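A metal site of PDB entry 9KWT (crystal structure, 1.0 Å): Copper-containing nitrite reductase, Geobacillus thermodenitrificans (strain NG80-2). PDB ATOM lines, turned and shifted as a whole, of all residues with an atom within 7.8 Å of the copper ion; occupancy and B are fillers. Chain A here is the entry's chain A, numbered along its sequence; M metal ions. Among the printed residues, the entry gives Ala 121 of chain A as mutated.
The copper ion is bound by a ring nitrogen (ND1) of His 80 (2.0 Å), a ring nitrogen (ND1) of His 128 (2.0 Å), the side-chain sulfur of Cys 120 (2.2 Å) and the side-chain sulfur of Met 133 (2.6 Å).
N of His 80 sits close to ND2 of Asn 73 (3.5 Å). The backbone NH of Met 133 lies close to the backbone carbonyl oxygen of Trp 48 (3.3 Å). The side-chain carboxylate (OD2) of Asp 75 lies within hydrogen-bond range of a ring nitrogen (NE2) of His 80 (2.8 Å). The side-chain sulfur of Cys 120 lies close to the side-chain hydroxyl of Thr 122 (3.4 Å). The backbone NH of Ser 81 sits close to the side-chain sulfur of Cys 120. NE2 of His 80 lies close to O of Val 78, 3.4 Å away.
Within 4 Å of the copper ion: His 80, Cys 120, His 128 and Met 133. The nearest printed residue that does not touch the copper ion is Pro 79 (4.03 Å).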
ATOM      1  N   ALA A  32     -17.124   9.261  16.679  1.00  0.00           N
ATOM      2  CA  ALA A  32     -17.669   9.491  18.017  1.00  0.00           C
ATOM      3  C   ALA A  32     -16.683   8.850  18.987  1.00  0.00           C
ATOM      4  O   ALA A  32     -16.323   7.680  18.813  1.00  0.00           O
ATOM      5  CB  ALA A  32     -19.054   8.882  18.189  1.00  0.00           C
ATOM      6  N   TRP A  48     -18.188  13.172  25.786  1.00  0.00           N
ATOM      7  CA  TRP A  48     -18.647  12.466  24.607  1.00  0.00           C
ATOM      8  C   TRP A  48     -18.473  13.435  23.447  1.00  0.00           C
ATOM      9  O   TRP A  48     -18.999  14.562  23.502  1.00  0.00           O
ATOM     10  CB  TRP A  48     -20.113  12.075  24.760  1.00  0.00           C
ATOM     11  CG  TRP A  48     -20.454  11.181  25.917  1.00  0.00           C
ATOM     12  CD1 TRP A  48     -19.672  10.775  26.965  1.00  0.00           C
ATOM     13  CD2 TRP A  48     -21.740  10.585  26.120  1.00  0.00           C
ATOM     14  NE1 TRP A  48     -20.398   9.959  27.804  1.00  0.00           N
ATOM     15  CE2 TRP A  48     -21.674   9.826  27.306  1.00  0.00           C
ATOM     16  CE3 TRP A  48     -22.955  10.650  25.435  1.00  0.00           C
ATOM     17  CZ2 TRP A  48     -22.768   9.132  27.802  1.00  0.00           C
ATOM     18  CZ3 TRP A  48     -24.034   9.972  25.937  1.00  0.00           C
ATOM     19  CH2 TRP A  48     -23.943   9.207  27.106  1.00  0.00           C
ATOM     20  N   THR A  49     -17.739  13.025  22.417  1.00  0.00           N
ATOM     21  CA  THR A  49     -17.273  13.977  21.412  1.00  0.00           C
ATOM     22  C   THR A  49     -17.381  13.420  20.006  1.00  0.00           C
ATOM     23  O   THR A  49     -17.408  12.204  19.790  1.00  0.00           O
ATOM     24  CB  THR A  49     -15.805  14.386  21.615  1.00  0.00           C
ATOM     25  OG1 THR A  49     -14.937  13.323  21.191  1.00  0.00           O
ATOM     26  CG2 THR A  49     -15.514  14.763  23.049  1.00  0.00           C
ATOM     27  N   PHE A  50     -17.351  14.346  19.062  1.00  0.00           N
ATOM     28  CA  PHE A  50     -16.914  14.066  17.710  1.00  0.00           C
ATOM     29  C   PHE A  50     -15.427  14.384  17.619  1.00  0.00           C
ATOM     30  O   PHE A  50     -15.001  15.521  17.895  1.00  0.00           O
ATOM     31  CB  PHE A  50     -17.703  14.905  16.707  1.00  0.00           C
ATOM     32  CG  PHE A  50     -19.180  14.584  16.695  1.00  0.00           C
ATOM     33  CD1 PHE A  50     -19.642  13.414  16.137  1.00  0.00           C
ATOM     34  CD2 PHE A  50     -20.089  15.461  17.277  1.00  0.00           C
ATOM     35  CE1 PHE A  50     -21.003  13.128  16.131  1.00  0.00           C
ATOM     36  CE2 PHE A  50     -21.447  15.166  17.266  1.00  0.00           C
ATOM     37  CZ  PHE A  50     -21.898  14.004  16.678  1.00  0.00           C
ATOM     38  N   LEU A  71     -19.892   8.304  10.049  1.00  0.00           N
ATOM     39  CA  LEU A  71     -19.564   8.328  11.474  1.00  0.00           C
ATOM     40  C   LEU A  71     -18.988   6.984  11.866  1.00  0.00           C
ATOM     41  O   LEU A  71     -19.634   5.953  11.674  1.00  0.00           O
ATOM     42  CB  LEU A  71     -20.810   8.611  12.309  1.00  0.00           C
ATOM     43  CG  LEU A  71     -20.569   8.760  13.815  1.00  0.00           C
ATOM     44  CD1 LEU A  71     -19.702   9.971  14.120  1.00  0.00           C
ATOM     45  CD2 LEU A  71     -21.897   8.859  14.544  1.00  0.00           C
ATOM     46  N   ASN A  73     -18.040   5.022  15.086  1.00  0.00           N
ATOM     47  CA  ASN A  73     -18.310   5.070  16.510  1.00  0.00           C
ATOM     48  C   ASN A  73     -17.234   4.294  17.283  1.00  0.00           C
ATOM     49  O   ASN A  73     -17.206   3.063  17.232  1.00  0.00           O
ATOM     50  CB  ASN A  73     -19.702   4.550  16.850  1.00  0.00           C
ATOM     51  CG  ASN A  73     -20.053   4.777  18.303  1.00  0.00           C
ATOM     52  OD1 ASN A  73     -19.264   5.341  19.058  1.00  0.00           O
ATOM     53  ND2 ASN A  73     -21.223   4.307  18.704  1.00  0.00           N
ATOM     54  N   ASP A  75     -16.905   4.718  20.639  1.00  0.00           N
ATOM     55  CA  ASP A  75     -17.373   4.509  21.999  1.00  0.00           C
ATOM     56  C   ASP A  75     -17.572   3.013  22.219  1.00  0.00           C
ATOM     57  O   ASP A  75     -18.213   2.360  21.385  1.00  0.00           O
ATOM     58  CB  ASP A  75     -18.700   5.259  22.165  1.00  0.00           C
ATOM     59  CG  ASP A  75     -19.236   5.298  23.598  1.00  0.00           C
ATOM     60  OD1 ASP A  75     -19.160   4.261  24.310  1.00  0.00           O
ATOM     61  OD2 ASP A  75     -19.778   6.353  24.000  1.00  0.00           O
ATOM     62  N   VAL A  78     -21.839   3.020  23.998  1.00  0.00           N
ATOM     63  CA  VAL A  78     -22.975   3.891  23.703  1.00  0.00           C
ATOM     64  C   VAL A  78     -23.097   4.107  22.198  1.00  0.00           C
ATOM     65  O   VAL A  78     -22.109   4.492  21.560  1.00  0.00           O
ATOM     66  CB  VAL A  78     -22.897   5.239  24.439  1.00  0.00           C
ATOM     67  CG1 VAL A  78     -24.208   5.997  24.284  1.00  0.00           C
ATOM     68  CG2 VAL A  78     -22.561   5.060  25.909  1.00  0.00           C
ATOM     69  N   PRO A  79     -24.280   3.897  21.599  1.00  0.00           N
ATOM     70  CA  PRO A  79     -24.498   4.312  20.212  1.00  0.00           C
ATOM     71  C   PRO A  79     -24.437   5.839  20.076  1.00  0.00           C
ATOM     72  O   PRO A  79     -24.726   6.568  21.021  1.00  0.00           O
ATOM     73  CB  PRO A  79     -25.908   3.805  19.900  1.00  0.00           C
ATOM     74  CG  PRO A  79     -26.175   2.742  20.933  1.00  0.00           C
ATOM     75  CD  PRO A  79     -25.486   3.258  22.154  1.00  0.00           C
ATOM     76  N   HIS A  80     -24.090   6.300  18.873  1.00  0.00           N
ATOM     77  CA  HIS A  80     -24.079   7.720  18.555  1.00  0.00           C
ATOM     78  C   HIS A  80     -24.582   7.932  17.139  1.00  0.00           C
ATOM     79  O   HIS A  80     -24.715   6.998  16.354  1.00  0.00           O
ATOM     80  CB  HIS A  80     -22.686   8.335  18.742  1.00  0.00           C
ATOM     81  CG  HIS A  80     -22.208   8.247  20.154  1.00  0.00           C
ATOM     82  ND1 HIS A  80     -22.752   9.010  21.173  1.00  0.00           N
ATOM     83  CD2 HIS A  80     -21.274   7.446  20.726  1.00  0.00           C
ATOM     84  CE1 HIS A  80     -22.148   8.691  22.303  1.00  0.00           C
ATOM     85  NE2 HIS A  80     -21.261   7.732  22.063  1.00  0.00           N
ATOM     86  N   SER A  81     -24.844   9.198  16.802  1.00  0.00           N
ATOM     87  CA  SER A  81     -25.454   9.542  15.529  1.00  0.00           C
ATOM     88  C   SER A  81     -25.090  10.995  15.205  1.00  0.00           C
ATOM     89  O   SER A  81     -24.396  11.667  15.977  1.00  0.00           O
ATOM     90  CB  SER A  81     -26.974   9.403  15.598  1.00  0.00           C
ATOM     91  OG  SER A  81     -27.502  10.201  16.655  1.00  0.00           O
ATOM     92  N   MET A  82     -25.582  11.476  14.066  1.00  0.00           N
ATOM     93  CA  MET A  82     -25.300  12.835  13.626  1.00  0.00           C
ATOM     94  C   MET A  82     -26.530  13.468  12.998  1.00  0.00           C
ATOM     95  O   MET A  82     -27.152  12.894  12.100  1.00  0.00           O
ATOM     96  CB  MET A  82     -24.168  12.851  12.591  1.00  0.00           C
ATOM     97  CG  MET A  82     -23.910  14.209  11.951  1.00  0.00           C
ATOM     98  SD  MET A  82     -23.386  15.484  13.136  1.00  0.00           S
ATOM     99  CE  MET A  82     -21.623  15.114  13.196  1.00  0.00           C
ATOM    100  N   ASP A  97     -28.744   5.751  14.585  1.00  0.00           N
ATOM    101  CA  ASP A  97     -27.622   5.356  15.407  1.00  0.00           C
ATOM    102  C   ASP A  97     -26.624   4.488  14.653  1.00  0.00           C
ATOM    103  O   ASP A  97     -26.967   3.675  13.791  1.00  0.00           O
ATOM    104  CB  ASP A  97     -28.121   4.580  16.624  1.00  0.00           C
ATOM    105  CG  ASP A  97     -28.808   5.467  17.639  1.00  0.00           C
ATOM    106  OD1 ASP A  97     -28.688   6.710  17.558  1.00  0.00           O
ATOM    107  OD2 ASP A  97     -29.510   4.918  18.517  1.00  0.00           O
ATOM    108  N   HIS A 119     -25.045  18.052  15.829  1.00  0.00           N
ATOM    109  CA  HIS A 119     -24.987  17.400  17.124  1.00  0.00           C
ATOM    110  C   HIS A 119     -25.400  15.936  16.999  1.00  0.00           C
ATOM    111  O   HIS A 119     -26.051  15.541  16.036  1.00  0.00           O
ATOM    112  CB  HIS A 119     -25.908  18.113  18.141  1.00  0.00           C
ATOM    113  CG  HIS A 119     -27.339  18.175  17.720  1.00  0.00           C
ATOM    114  ND1 HIS A 119     -28.238  17.166  17.964  1.00  0.00           N
ATOM    115  CD2 HIS A 119     -28.044  19.152  17.092  1.00  0.00           C
ATOM    116  CE1 HIS A 119     -29.435  17.525  17.512  1.00  0.00           C
ATOM    117  NE2 HIS A 119     -29.338  18.718  16.962  1.00  0.00           N
ATOM    118  N   CYS A 120     -25.066  15.161  18.018  1.00  0.00           N
ATOM    119  CA  CYS A 120     -25.559  13.801  18.086  1.00  0.00           C
ATOM    120  C   CYS A 120     -27.075  13.816  18.299  1.00  0.00           C
ATOM    121  O   CYS A 120     -27.616  14.683  18.988  1.00  0.00           O
ATOM    122  CB  CYS A 120     -24.830  13.065  19.212  1.00  0.00           C
ATOM    123  SG  CYS A 120     -25.373  11.368  19.442  1.00  0.00           S
ATOM    124  N   ALA A 121     -27.740  12.827  17.692  1.00  0.00           N
ATOM    125  CA  ALA A 121     -29.186  12.719  17.647  1.00  0.00           C
ATOM    126  C   ALA A 121     -29.704  11.508  18.417  1.00  0.00           C
ATOM    127  O   ALA A 121     -30.869  11.141  18.242  1.00  0.00           O
ATOM    128  CB  ALA A 121     -29.670  12.661  16.186  1.00  0.00           C
ATOM    129  N   THR A 122     -28.873  10.861  19.231  1.00  0.00           N
ATOM    130  CA  THR A 122     -29.259   9.636  19.904  1.00  0.00           C
ATOM    131  C   THR A 122     -30.013   9.950  21.190  1.00  0.00           C
ATOM    132  O   THR A 122     -29.646  10.838  21.952  1.00  0.00           O
ATOM    133  CB  THR A 122     -27.982   8.847  20.204  1.00  0.00           C
ATOM    134  OG1 THR A 122     -27.307   8.561  18.961  1.00  0.00           O
ATOM    135  CG2 THR A 122     -28.254   7.556  20.957  1.00  0.00           C
ATOM    136  N   LYS A 123     -31.095   9.202  21.434  1.00  0.00           N
ATOM    137  CA  LYS A 123     -31.912   9.424  22.614  1.00  0.00           C
ATOM    138  C   LYS A 123     -31.164   8.945  23.864  1.00  0.00           C
ATOM    139  O   LYS A 123     -30.563   7.861  23.857  1.00  0.00           O
ATOM    140  CB  LYS A 123     -33.233   8.660  22.491  1.00  0.00           C
ATOM    141  CG  LYS A 123     -34.125   8.697  23.732  1.00  0.00           C
ATOM    142  CD  LYS A 123     -35.613   8.490  23.385  1.00  0.00           C
ATOM    143  CE  LYS A 123     -36.477   8.365  24.633  1.00  0.00           C
ATOM    144  NZ  LYS A 123     -36.936   6.982  24.887  1.00  0.00           N
ATOM    145  N   PRO A 124     -31.201   9.707  24.971  1.00  0.00           N
ATOM    146  CA  PRO A 124     -31.784  11.052  25.116  1.00  0.00           C
ATOM    147  C   PRO A 124     -30.867  12.103  24.511  1.00  0.00           C
ATOM    148  O   PRO A 124     -29.679  12.189  24.870  1.00  0.00           O
ATOM    149  CB  PRO A 124     -31.885  11.254  26.635  1.00  0.00           C
ATOM    150  CG  PRO A 124     -31.459   9.994  27.250  1.00  0.00           C
ATOM    151  CD  PRO A 124     -30.693   9.205  26.254  1.00  0.00           C
ATOM    152  N   VAL A 125     -31.401  12.899  23.587  1.00  0.00           N
ATOM    153  CA  VAL A 125     -30.569  13.856  22.887  1.00  0.00           C
ATOM    154  C   VAL A 125     -29.928  14.844  23.864  1.00  0.00           C
ATOM    155  O   VAL A 125     -28.758  15.225  23.699  1.00  0.00           O
ATOM    156  CB  VAL A 125     -31.370  14.556  21.773  1.00  0.00           C
ATOM    157  CG1 VAL A 125     -30.561  15.652  21.110  1.00  0.00           C
ATOM    158  CG2 VAL A 125     -31.818  13.525  20.735  1.00  0.00           C
ATOM    159  N   GLN A 127     -28.790  14.288  26.753  1.00  0.00           N
ATOM    160  CA  GLN A 127     -27.605  13.667  27.346  1.00  0.00           C
ATOM    161  C   GLN A 127     -26.411  13.726  26.394  1.00  0.00           C
ATOM    162  O   GLN A 127     -25.289  14.035  26.802  1.00  0.00           O
ATOM    163  CB  GLN A 127     -27.931  12.215  27.722  1.00  0.00           C
ATOM    164  CG  GLN A 127     -26.817  11.520  28.464  1.00  0.00           C
ATOM    165  CD  GLN A 127     -27.200  10.138  28.936  1.00  0.00           C
ATOM    166  OE1 GLN A 127     -28.170   9.556  28.457  1.00  0.00           O
ATOM    167  NE2 GLN A 127     -26.440   9.618  29.885  1.00  0.00           N
ATOM    168  N   HIS A 128     -26.639  13.398  25.123  1.00  0.00           N
ATOM    169  CA  HIS A 128     -25.555  13.377  24.164  1.00  0.00           C
ATOM    170  C   HIS A 128     -25.025  14.778  23.889  1.00  0.00           C
ATOM    171  O   HIS A 128     -23.806  14.977  23.809  1.00  0.00           O
ATOM    172  CB  HIS A 128     -25.990  12.656  22.897  1.00  0.00           C
ATOM    173  CG  HIS A 128     -26.141  11.187  23.081  1.00  0.00           C
ATOM    174  ND1 HIS A 128     -25.218  10.283  22.585  1.00  0.00           N
ATOM    175  CD2 HIS A 128     -27.058  10.460  23.757  1.00  0.00           C
ATOM    176  CE1 HIS A 128     -25.595   9.064  22.913  1.00  0.00           C
ATOM    177  NE2 HIS A 128     -26.704   9.150  23.638  1.00  0.00           N
ATOM    178  N   ILE A 129     -25.920  15.769  23.743  1.00  0.00           N
ATOM    179  CA  ILE A 129     -25.454  17.142  23.561  1.00  0.00           C
ATOM    180  C   ILE A 129     -24.724  17.625  24.807  1.00  0.00           C
ATOM    181  O   ILE A 129     -23.604  18.150  24.718  1.00  0.00           O
ATOM    182  CB  ILE A 129     -26.621  18.086  23.193  1.00  0.00           C
ATOM    183  CG1 ILE A 129     -27.275  17.674  21.875  1.00  0.00           C
ATOM    184  CG2 ILE A 129     -26.088  19.518  23.090  1.00  0.00           C
ATOM    185  CD1 ILE A 129     -28.469  18.556  21.468  1.00  0.00           C
ATOM    186  N   ASN A 131     -23.160  16.165  27.121  1.00  0.00           N
ATOM    187  CA  ASN A 131     -21.855  15.547  27.347  1.00  0.00           C
ATOM    188  C   ASN A 131     -20.804  15.944  26.329  1.00  0.00           C
ATOM    189  O   ASN A 131     -19.634  15.582  26.513  1.00  0.00           O
ATOM    190  CB  ASN A 131     -21.973  14.023  27.389  1.00  0.00           C
ATOM    191  CG  ASN A 131     -22.493  13.503  28.724  1.00  0.00           C
ATOM    192  OD1 ASN A 131     -22.208  14.047  29.794  1.00  0.00           O
ATOM    193  ND2 ASN A 131     -23.225  12.411  28.666  1.00  0.00           N
ATOM    194  N   GLY A 132     -21.158  16.721  25.290  1.00  0.00           N
ATOM    195  CA  GLY A 132     -20.183  17.315  24.408  1.00  0.00           C
ATOM    196  C   GLY A 132     -20.409  17.148  22.926  1.00  0.00           C
ATOM    197  O   GLY A 132     -19.607  17.663  22.145  1.00  0.00           O
ATOM    198  N   MET A 133     -21.473  16.459  22.504  1.00  0.00           N
ATOM    199  CA  MET A 133     -21.634  16.102  21.090  1.00  0.00           C
ATOM    200  C   MET A 133     -22.392  17.173  20.311  1.00  0.00           C
ATOM    201  O   MET A 133     -23.538  16.984  19.908  1.00  0.00           O
ATOM    202  CB  MET A 133     -22.234  14.720  20.910  1.00  0.00           C
ATOM    203  CG  MET A 133     -21.508  13.670  21.714  1.00  0.00           C
ATOM    204  SD  MET A 133     -21.896  11.945  21.323  1.00  0.00           S
ATOM    205  CE  MET A 133     -21.047  11.790  19.771  1.00  0.00           C
HETATM  206 CU    CU M   1     -24.027  10.541  20.982  1.00  0.00          CU
